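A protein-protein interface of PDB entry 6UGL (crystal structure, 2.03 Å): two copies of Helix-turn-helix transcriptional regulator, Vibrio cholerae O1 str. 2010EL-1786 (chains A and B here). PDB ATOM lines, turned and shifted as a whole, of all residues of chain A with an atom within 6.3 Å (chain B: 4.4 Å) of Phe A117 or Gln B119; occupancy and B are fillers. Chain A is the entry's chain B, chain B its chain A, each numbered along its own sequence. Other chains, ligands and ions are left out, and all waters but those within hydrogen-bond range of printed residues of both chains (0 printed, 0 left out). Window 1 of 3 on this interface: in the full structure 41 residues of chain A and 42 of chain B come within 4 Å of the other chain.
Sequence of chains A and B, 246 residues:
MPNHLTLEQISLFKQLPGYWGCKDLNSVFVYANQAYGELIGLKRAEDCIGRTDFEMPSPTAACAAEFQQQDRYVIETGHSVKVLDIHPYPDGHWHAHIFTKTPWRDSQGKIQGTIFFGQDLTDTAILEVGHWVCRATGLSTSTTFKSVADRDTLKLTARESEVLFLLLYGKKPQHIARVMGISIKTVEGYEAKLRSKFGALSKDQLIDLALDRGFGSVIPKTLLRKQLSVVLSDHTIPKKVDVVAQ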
ATOM      1  N   LEU A  16     -21.583 -30.902  -8.483  1.00  0.00           N
ATOM      2  CA  LEU A  16     -20.480 -30.071  -8.951  1.00  0.00           C
ATOM      3  C   LEU A  16     -20.451 -28.766  -8.158  1.00  0.00           C
ATOM      4  O   LEU A  16     -21.504 -28.183  -7.908  1.00  0.00           O
ATOM      5  CB  LEU A  16     -20.630 -29.757 -10.442  1.00  0.00           C
ATOM      6  CG  LEU A  16     -20.375 -30.844 -11.486  1.00  0.00           C
ATOM      7  CD1 LEU A  16     -20.849 -30.367 -12.845  1.00  0.00           C
ATOM      8  CD2 LEU A  16     -18.912 -31.172 -11.549  1.00  0.00           C
ATOM      9  N   PRO A  17     -19.281 -28.285  -7.743  1.00  0.00           N
ATOM     10  CA  PRO A  17     -19.236 -27.084  -6.898  1.00  0.00           C
ATOM     11  C   PRO A  17     -19.604 -25.832  -7.680  1.00  0.00           C
ATOM     12  O   PRO A  17     -19.744 -25.827  -8.907  1.00  0.00           O
ATOM     13  CB  PRO A  17     -17.778 -27.040  -6.419  1.00  0.00           C
ATOM     14  CG  PRO A  17     -17.019 -27.746  -7.482  1.00  0.00           C
ATOM     15  CD  PRO A  17     -17.939 -28.860  -7.943  1.00  0.00           C
ATOM     16  N   GLY A  18     -19.733 -24.746  -6.938  1.00  0.00           N
ATOM     17  CA  GLY A  18     -20.149 -23.489  -7.515  1.00  0.00           C
ATOM     18  C   GLY A  18     -21.649 -23.268  -7.393  1.00  0.00           C
ATOM     19  O   GLY A  18     -22.416 -24.116  -6.936  1.00  0.00           O
ATOM     20  N   TYR A  19     -22.056 -22.080  -7.819  1.00  0.00           N
ATOM     21  CA  TYR A  19     -23.449 -21.670  -7.929  1.00  0.00           C
ATOM     22  C   TYR A  19     -23.679 -21.310  -9.389  1.00  0.00           C
ATOM     23  O   TYR A  19     -23.174 -20.278  -9.862  1.00  0.00           O
ATOM     24  CB  TYR A  19     -23.740 -20.483  -7.009  1.00  0.00           C
ATOM     25  CG  TYR A  19     -23.125 -20.593  -5.636  1.00  0.00           C
ATOM     26  CD1 TYR A  19     -21.810 -20.212  -5.404  1.00  0.00           C
ATOM     27  CD2 TYR A  19     -23.861 -21.070  -4.572  1.00  0.00           C
ATOM     28  CE1 TYR A  19     -21.244 -20.316  -4.146  1.00  0.00           C
ATOM     29  CE2 TYR A  19     -23.313 -21.163  -3.308  1.00  0.00           C
ATOM     30  CZ  TYR A  19     -21.992 -20.798  -3.104  1.00  0.00           C
ATOM     31  OH  TYR A  19     -21.451 -20.896  -1.842  1.00  0.00           O
ATOM     32  N   TRP A  20     -24.400 -22.165 -10.116  1.00  0.00           N
ATOM     33  CA  TRP A  20     -24.409 -22.066 -11.569  1.00  0.00           C
ATOM     34  C   TRP A  20     -25.760 -22.472 -12.152  1.00  0.00           C
ATOM     35  O   TRP A  20     -26.630 -23.017 -11.466  1.00  0.00           O
ATOM     36  CB  TRP A  20     -23.277 -22.900 -12.194  1.00  0.00           C
ATOM     37  CG  TRP A  20     -23.146 -24.328 -11.701  1.00  0.00           C
ATOM     38  CD1 TRP A  20     -22.302 -24.779 -10.735  1.00  0.00           C
ATOM     39  CD2 TRP A  20     -23.856 -25.480 -12.185  1.00  0.00           C
ATOM     40  NE1 TRP A  20     -22.446 -26.138 -10.572  1.00  0.00           N
ATOM     41  CE2 TRP A  20     -23.395 -26.592 -11.450  1.00  0.00           C
ATOM     42  CE3 TRP A  20     -24.845 -25.675 -13.162  1.00  0.00           C
ATOM     43  CZ2 TRP A  20     -23.884 -27.880 -11.659  1.00  0.00           C
ATOM     44  CZ3 TRP A  20     -25.321 -26.957 -13.376  1.00  0.00           C
ATOM     45  CH2 TRP A  20     -24.845 -28.045 -12.626  1.00  0.00           C
ATOM     46  N   GLY A  21     -25.918 -22.159 -13.435  1.00  0.00           N
ATOM     47  CA  GLY A  21     -27.077 -22.548 -14.216  1.00  0.00           C
ATOM     48  C   GLY A  21     -26.992 -21.879 -15.576  1.00  0.00           C
ATOM     49  O   GLY A  21     -25.950 -21.339 -15.942  1.00  0.00           O
ATOM     50  N   LYS A  82     -16.081 -11.840 -16.424  1.00  0.00           N
ATOM     51  CA  LYS A  82     -16.051 -12.108 -14.996  1.00  0.00           C
ATOM     52  C   LYS A  82     -16.624 -10.909 -14.252  1.00  0.00           C
ATOM     53  O   LYS A  82     -16.283  -9.759 -14.549  1.00  0.00           O
ATOM     54  CB  LYS A  82     -14.629 -12.428 -14.518  1.00  0.00           C
ATOM     55  CG  LYS A  82     -14.135 -13.803 -15.004  1.00  0.00           C
ATOM     56  CD  LYS A  82     -12.874 -14.263 -14.276  1.00  0.00           C
ATOM     57  CE  LYS A  82     -12.488 -15.680 -14.704  1.00  0.00           C
ATOM     58  NZ  LYS A  82     -11.608 -16.370 -13.716  1.00  0.00           N
ATOM     59  N   ILE A  98     -17.403 -14.227  -7.396  1.00  0.00           N
ATOM     60  CA  ILE A  98     -17.077 -13.975  -8.788  1.00  0.00           C
ATOM     61  C   ILE A  98     -18.028 -14.805  -9.643  1.00  0.00           C
ATOM     62  O   ILE A  98     -18.113 -16.031  -9.488  1.00  0.00           O
ATOM     63  CB  ILE A  98     -15.616 -14.318  -9.100  1.00  0.00           C
ATOM     64  CG1 ILE A  98     -14.666 -13.570  -8.152  1.00  0.00           C
ATOM     65  CG2 ILE A  98     -15.321 -14.033 -10.578  1.00  0.00           C
ATOM     66  CD1 ILE A  98     -14.500 -12.124  -8.489  1.00  0.00           C
ATOM     67  N   PHE A  99     -18.732 -14.144 -10.551  1.00  0.00           N
ATOM     68  CA  PHE A  99     -19.601 -14.815 -11.506  1.00  0.00           C
ATOM     69  C   PHE A  99     -18.996 -14.715 -12.897  1.00  0.00           C
ATOM     70  O   PHE A  99     -18.727 -13.613 -13.386  1.00  0.00           O
ATOM     71  CB  PHE A  99     -21.015 -14.226 -11.473  1.00  0.00           C
ATOM     72  CG  PHE A  99     -21.912 -14.870 -10.432  1.00  0.00           C
ATOM     73  CD1 PHE A  99     -22.650 -16.012 -10.738  1.00  0.00           C
ATOM     74  CD2 PHE A  99     -22.002 -14.347  -9.147  1.00  0.00           C
ATOM     75  CE1 PHE A  99     -23.463 -16.616  -9.785  1.00  0.00           C
ATOM     76  CE2 PHE A  99     -22.802 -14.938  -8.191  1.00  0.00           C
ATOM     77  CZ  PHE A  99     -23.542 -16.083  -8.510  1.00  0.00           C
ATOM     78  N   THR A 100     -18.767 -15.868 -13.520  1.00  0.00           N
ATOM     79  CA  THR A 100     -18.330 -15.952 -14.902  1.00  0.00           C
ATOM     80  C   THR A 100     -19.533 -16.243 -15.794  1.00  0.00           C
ATOM     81  O   THR A 100     -20.371 -17.093 -15.468  1.00  0.00           O
ATOM     82  CB  THR A 100     -17.266 -17.045 -15.051  1.00  0.00           C
ATOM     83  OG1 THR A 100     -16.171 -16.740 -14.174  1.00  0.00           O
ATOM     84  CG2 THR A 100     -16.780 -17.138 -16.476  1.00  0.00           C
ATOM     85  N   LYS A 101     -19.632 -15.517 -16.907  1.00  0.00           N
ATOM     86  CA  LYS A 101     -20.753 -15.670 -17.817  1.00  0.00           C
ATOM     87  C   LYS A 101     -20.219 -16.006 -19.195  1.00  0.00           C
ATOM     88  O   LYS A 101     -19.375 -15.285 -19.734  1.00  0.00           O
ATOM     89  CB  LYS A 101     -21.643 -14.407 -17.852  1.00  0.00           C
ATOM     90  CG  LYS A 101     -22.367 -14.151 -16.521  1.00  0.00           C
ATOM     91  CD  LYS A 101     -23.115 -12.819 -16.459  1.00  0.00           C
ATOM     92  CE  LYS A 101     -23.988 -12.778 -15.200  1.00  0.00           C
ATOM     93  NZ  LYS A 101     -25.045 -11.727 -15.199  1.00  0.00           N
ATOM     94  N   ILE A 115     -24.584 -19.149 -19.876  1.00  0.00           N
ATOM     95  CA  ILE A 115     -24.227 -19.965 -18.721  1.00  0.00           C
ATOM     96  C   ILE A 115     -23.581 -19.057 -17.680  1.00  0.00           C
ATOM     97  O   ILE A 115     -22.700 -18.252 -18.012  1.00  0.00           O
ATOM     98  CB  ILE A 115     -23.252 -21.085 -19.121  1.00  0.00           C
ATOM     99  CG1 ILE A 115     -23.905 -22.082 -20.082  1.00  0.00           C
ATOM    100  CG2 ILE A 115     -22.680 -21.768 -17.886  1.00  0.00           C
ATOM    101  CD1 ILE A 115     -22.881 -23.047 -20.759  1.00  0.00           C
ATOM    102  N   PHE A 116     -23.971 -19.212 -16.422  1.00  0.00           N
ATOM    103  CA  PHE A 116     -23.395 -18.445 -15.331  1.00  0.00           C
ATOM    104  C   PHE A 116     -22.834 -19.407 -14.307  1.00  0.00           C
ATOM    105  O   PHE A 116     -23.448 -20.441 -14.027  1.00  0.00           O
ATOM    106  CB  PHE A 116     -24.424 -17.482 -14.666  1.00  0.00           C
ATOM    107  CG  PHE A 116     -25.577 -18.180 -13.964  1.00  0.00           C
ATOM    108  CD1 PHE A 116     -25.456 -18.602 -12.644  1.00  0.00           C
ATOM    109  CD2 PHE A 116     -26.787 -18.385 -14.619  1.00  0.00           C
ATOM    110  CE1 PHE A 116     -26.495 -19.257 -12.004  1.00  0.00           C
ATOM    111  CE2 PHE A 116     -27.854 -19.031 -13.979  1.00  0.00           C
ATOM    112  CZ  PHE A 116     -27.704 -19.467 -12.668  1.00  0.00           C
ATOM    113  N   PHE A 117     -21.667 -19.050 -13.756  1.00  0.00           N
ATOM    114  CA  PHE A 117     -20.952 -19.883 -12.793  1.00  0.00           C
ATOM    115  C   PHE A 117     -20.324 -18.981 -11.735  1.00  0.00           C
ATOM    116  O   PHE A 117     -19.380 -18.239 -12.031  1.00  0.00           O
ATOM    117  CB  PHE A 117     -19.873 -20.734 -13.477  1.00  0.00           C
ATOM    118  CG  PHE A 117     -19.130 -21.638 -12.524  1.00  0.00           C
ATOM    119  CD1 PHE A 117     -17.997 -21.196 -11.858  1.00  0.00           C
ATOM    120  CD2 PHE A 117     -19.583 -22.930 -12.280  1.00  0.00           C
ATOM    121  CE1 PHE A 117     -17.331 -22.024 -10.975  1.00  0.00           C
ATOM    122  CE2 PHE A 117     -18.940 -23.754 -11.394  1.00  0.00           C
ATOM    123  CZ  PHE A 117     -17.795 -23.310 -10.745  1.00  0.00           C
ATOM    124  N   GLY A 118     -20.789 -19.101 -10.498  1.00  0.00           N
ATOM    125  CA  GLY A 118     -20.330 -18.263  -9.397  1.00  0.00           C
ATOM    126  C   GLY A 118     -19.458 -19.020  -8.411  1.00  0.00           C
ATOM    127  O   GLY A 118     -19.715 -20.192  -8.108  1.00  0.00           O
ATOM    128  N   GLN A 119     -18.437 -18.330  -7.901  1.00  0.00           N
ATOM    129  CA  GLN A 119     -17.556 -18.835  -6.856  1.00  0.00           C
ATOM    130  C   GLN A 119     -17.642 -17.917  -5.650  1.00  0.00           C
ATOM    131  O   GLN A 119     -17.656 -16.693  -5.805  1.00  0.00           O
ATOM    132  CB  GLN A 119     -16.083 -18.883  -7.311  1.00  0.00           C
ATOM    133  CG  GLN A 119     -15.839 -19.492  -8.673  1.00  0.00           C
ATOM    134  CD  GLN A 119     -14.388 -19.332  -9.123  1.00  0.00           C
ATOM    135  OE1 GLN A 119     -14.108 -18.680 -10.126  1.00  0.00           O
ATOM    136  NE2 GLN A 119     -13.465 -19.924  -8.374  1.00  0.00           N
ATOM    137  N   GLU A 128      -7.384 -15.828  -8.940  1.00  0.00           N
ATOM    138  CA  GLU A 128      -7.753 -16.144 -10.317  1.00  0.00           C
ATOM    139  C   GLU A 128      -8.069 -14.894 -11.124  1.00  0.00           C
ATOM    140  O   GLU A 128      -7.829 -14.865 -12.335  1.00  0.00           O
ATOM    141  CB  GLU A 128      -8.960 -17.090 -10.344  1.00  0.00           C
ATOM    142  CG  GLU A 128      -8.750 -18.394  -9.601  1.00  0.00           C
ATOM    143  CD  GLU A 128      -9.916 -19.353  -9.759  1.00  0.00           C
ATOM    144  OE1 GLU A 128     -10.641 -19.253 -10.771  1.00  0.00           O
ATOM    145  OE2 GLU A 128     -10.104 -20.208  -8.870  1.00  0.00           O
ATOM    146  N   LEU B  16     -20.840 -26.736 -19.431  1.00  0.00           N
ATOM    147  CA  LEU B  16     -20.353 -26.039 -18.248  1.00  0.00           C
ATOM    148  C   LEU B  16     -18.834 -25.885 -18.347  1.00  0.00           C
ATOM    149  O   LEU B  16     -18.122 -26.899 -18.445  1.00  0.00           O
ATOM    150  CB  LEU B  16     -20.734 -26.805 -16.985  1.00  0.00           C
ATOM    151  CG  LEU B  16     -20.530 -26.094 -15.647  1.00  0.00           C
ATOM    152  CD1 LEU B  16     -21.513 -24.937 -15.493  1.00  0.00           C
ATOM    153  CD2 LEU B  16     -20.694 -27.078 -14.502  1.00  0.00           C
ATOM    154  N   GLY B  18     -14.764 -25.241 -17.714  1.00  0.00           N
ATOM    155  CA  GLY B  18     -13.852 -25.834 -16.760  1.00  0.00           C
ATOM    156  C   GLY B  18     -13.442 -27.239 -17.172  1.00  0.00           C
ATOM    157  O   GLY B  18     -13.810 -27.750 -18.233  1.00  0.00           O
ATOM    158  N   ALA B  96      -1.533 -23.838 -16.140  1.00  0.00           N
ATOM    159  CA  ALA B  96      -1.692 -23.677 -14.700  1.00  0.00           C
ATOM    160  C   ALA B  96      -3.169 -23.629 -14.352  1.00  0.00           C
ATOM    161  O   ALA B  96      -3.945 -22.919 -15.001  1.00  0.00           O
ATOM    162  CB  ALA B  96      -0.996 -22.403 -14.194  1.00  0.00           C
ATOM    163  N   HIS B  97      -3.558 -24.370 -13.321  1.00  0.00           N
ATOM    164  CA  HIS B  97      -4.948 -24.390 -12.908  1.00  0.00           C
ATOM    165  C   HIS B  97      -5.029 -24.351 -11.393  1.00  0.00           C
ATOM    166  O   HIS B  97      -4.103 -24.753 -10.690  1.00  0.00           O
ATOM    167  CB  HIS B  97      -5.702 -25.644 -13.376  1.00  0.00           C
ATOM    168  CG  HIS B  97      -5.707 -25.866 -14.858  1.00  0.00           C
ATOM    169  ND1 HIS B  97      -4.617 -26.365 -15.538  1.00  0.00           N
ATOM    170  CD2 HIS B  97      -6.698 -25.747 -15.776  1.00  0.00           C
ATOM    171  CE1 HIS B  97      -4.925 -26.513 -16.815  1.00  0.00           C
ATOM    172  NE2 HIS B  97      -6.179 -26.138 -16.988  1.00  0.00           N
ATOM    173  N   ILE B  98      -6.164 -23.871 -10.900  1.00  0.00           N
ATOM    174  CA  ILE B  98      -6.640 -24.223  -9.571  1.00  0.00           C
ATOM    175  C   ILE B  98      -7.697 -25.305  -9.739  1.00  0.00           C
ATOM    176  O   ILE B  98      -8.725 -25.076 -10.385  1.00  0.00           O
ATOM    177  CB  ILE B  98      -7.218 -23.019  -8.820  1.00  0.00           C
ATOM    178  CG1 ILE B  98      -6.199 -21.880  -8.753  1.00  0.00           C
ATOM    179  CG2 ILE B  98      -7.594 -23.442  -7.416  1.00  0.00           C
ATOM    180  CD1 ILE B  98      -5.039 -22.187  -7.850  1.00  0.00           C
ATOM    181  N   PHE B 117     -12.632 -30.062 -10.090  1.00  0.00           N
ATOM    182  CA  PHE B 117     -13.124 -28.985 -10.942  1.00  0.00           C
ATOM    183  C   PHE B 117     -11.979 -28.006 -11.114  1.00  0.00           C
ATOM    184  O   PHE B 117     -11.563 -27.365 -10.144  1.00  0.00           O
ATOM    185  CB  PHE B 117     -14.356 -28.301 -10.344  1.00  0.00           C
ATOM    186  CG  PHE B 117     -15.219 -27.635 -11.371  1.00  0.00           C
ATOM    187  CD1 PHE B 117     -14.748 -26.557 -12.096  1.00  0.00           C
ATOM    188  CD2 PHE B 117     -16.503 -28.089 -11.616  1.00  0.00           C
ATOM    189  CE1 PHE B 117     -15.526 -25.946 -13.051  1.00  0.00           C
ATOM    190  CE2 PHE B 117     -17.290 -27.474 -12.572  1.00  0.00           C
ATOM    191  CZ  PHE B 117     -16.792 -26.399 -13.295  1.00  0.00           C
ATOM    192  N   GLY B 118     -11.477 -27.899 -12.336  1.00  0.00           N
ATOM    193  CA  GLY B 118     -10.298 -27.109 -12.633  1.00  0.00           C
ATOM    194  C   GLY B 118     -10.660 -25.883 -13.450  1.00  0.00           C
ATOM    195  O   GLY B 118     -11.543 -25.937 -14.313  1.00  0.00           O
ATOM    196  N   GLN B 119      -9.962 -24.784 -13.171  1.00  0.00           N
ATOM    197  CA  GLN B 119     -10.086 -23.528 -13.900  1.00  0.00           C
ATOM    198  C   GLN B 119      -8.720 -23.063 -14.375  1.00  0.00           C
ATOM    199  O   GLN B 119      -7.748 -23.095 -13.619  1.00  0.00           O
ATOM    200  CB  GLN B 119     -10.710 -22.422 -13.017  1.00  0.00           C
ATOM    201  CG  GLN B 119     -12.068 -22.750 -12.452  1.00  0.00           C
ATOM    202  CD  GLN B 119     -13.182 -22.652 -13.484  1.00  0.00           C
ATOM    203  OE1 GLN B 119     -12.939 -22.640 -14.694  1.00  0.00           O
ATOM    204  NE2 GLN B 119     -14.424 -22.574 -13.001  1.00  0.00           N
ATOM    205  N   ASP B 120      -8.665 -22.598 -15.617  1.00  0.00           N
ATOM    206  CA  ASP B 120      -7.457 -21.973 -16.147  1.00  0.00           C
ATOM    207  C   ASP B 120      -7.043 -20.756 -15.336  1.00  0.00           C
ATOM    208  O   ASP B 120      -7.868 -19.904 -15.006  1.00  0.00           O
ATOM    209  CB  ASP B 120      -7.683 -21.532 -17.590  1.00  0.00           C
ATOM    210  CG  ASP B 120      -7.809 -22.696 -18.546  1.00  0.00           C
ATOM    211  OD1 ASP B 120      -6.925 -23.570 -18.524  1.00  0.00           O
ATOM    212  OD2 ASP B 120      -8.780 -22.720 -19.326  1.00  0.00           O
ATOM    213  N   LEU B 121      -5.744 -20.647 -15.058  1.00  0.00           N
ATOM    214  CA  LEU B 121      -5.166 -19.408 -14.553  1.00  0.00           C
ATOM    215  C   LEU B 121      -4.711 -18.581 -15.752  1.00  0.00           C
ATOM    216  O   LEU B 121      -3.698 -18.893 -16.386  1.00  0.00           O
ATOM    217  CB  LEU B 121      -4.023 -19.698 -13.590  1.00  0.00           C
ATOM    218  CG  LEU B 121      -4.497 -20.172 -12.218  1.00  0.00           C
ATOM    219  CD1 LEU B 121      -3.359 -20.810 -11.442  1.00  0.00           C
ATOM    220  CD2 LEU B 121      -5.092 -19.006 -11.429  1.00  0.00           C
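The backbone carbonyl oxygen of Ile B98 sits at hydrogen-bond distance from the backbone NH of Gln B119.
The backbone carbonyl oxygen (O) of Leu A16 sits at hydrogen-bond distance from the indole nitrogen (NE1) of Trp A20 (3.5 Å).
The backbone carbonyl oxygen (O) of Pro A17 sits at hydrogen-bond distance from the indole nitrogen (NE1) of Trp A20.
The backbone carbonyl oxygen (O) of Phe A117 lies within hydrogen-bond range of the backbone NH (N) of Thr A100 (2.9 Å).
NE2 of Gln A119 is in hydrogen-bond range of OE2 of Glu A128 (3.4 Å).
Among the printed residues, pairs that only touch across the chains: Leu A16 with Leu B16 (3.7 Å), Leu A16 with Phe B117 (3.9 Å), Pro A17 with Phe B117 (3.9 Å), Phe A117 with Phe B117 (3.9 Å), Phe A117 with Gln B119 (3.6 Å) and Glu A128 with Gln B119 (3.9 Å).
Of the printed residues of chain B, Leu A16 touches Leu B16 and Phe B117.
Printed residues of chain B within 4 Å of Pro A17: Phe B117 (3.9 Å).
Thr A100 touches none of the printed residues of chain B.
Of chain B, only Phe B117 and Gln B119 come within 4 Å of Phe A117.
Of the printed residues of chain A, Leu B16 touches Leu A16 (3.7 Å).
His B97 touches none of the printed residues of chain A.
Of the printed residues of chain A, Phe B117 touches Leu A16, Pro A17 and Phe A117.
Printed residues of chain A that touch a printed residue of chain B: Leu A16, Pro A17, Phe A117 and Glu A128.
Hydrophobic or aromatic side chains of chain A that line the printed part of chain B: Leu A16, Pro A17 and Phe A117.
Along chain A the printed residues that touch a printed residue of chain B span positions 16 to 128.
Of the 10 printed residues of chain B, 3 touch a printed residue of chain A.
Printed residues of chain B that touch a printed residue of chain A: Leu B16, Phe B117 and Gln B119.
Among the printed residues, no Asp or Glu carboxylate lies within 4 Å of a Lys or Arg side-chain nitrogen of the other chain.
Leu A16 touches its own counterpart, Leu B16.
Leu A16 touches Phe B117, but with the chains exchanged Phe A117 does not touch Leu B16 (4.3 Å).
Phe A117 touches its own counterpart, Phe B117.
Phe A117 touches Gln B119, but with the chains exchanged Gln A119 does not touch Phe B117 (7.7 Å).
Positions printed for both chains: 16, 18, 98, 117, 118 and 119.
Of the 6 pairs that touch across the chains among the printed residues, 2 have their exchanged pair printed and touching as well.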
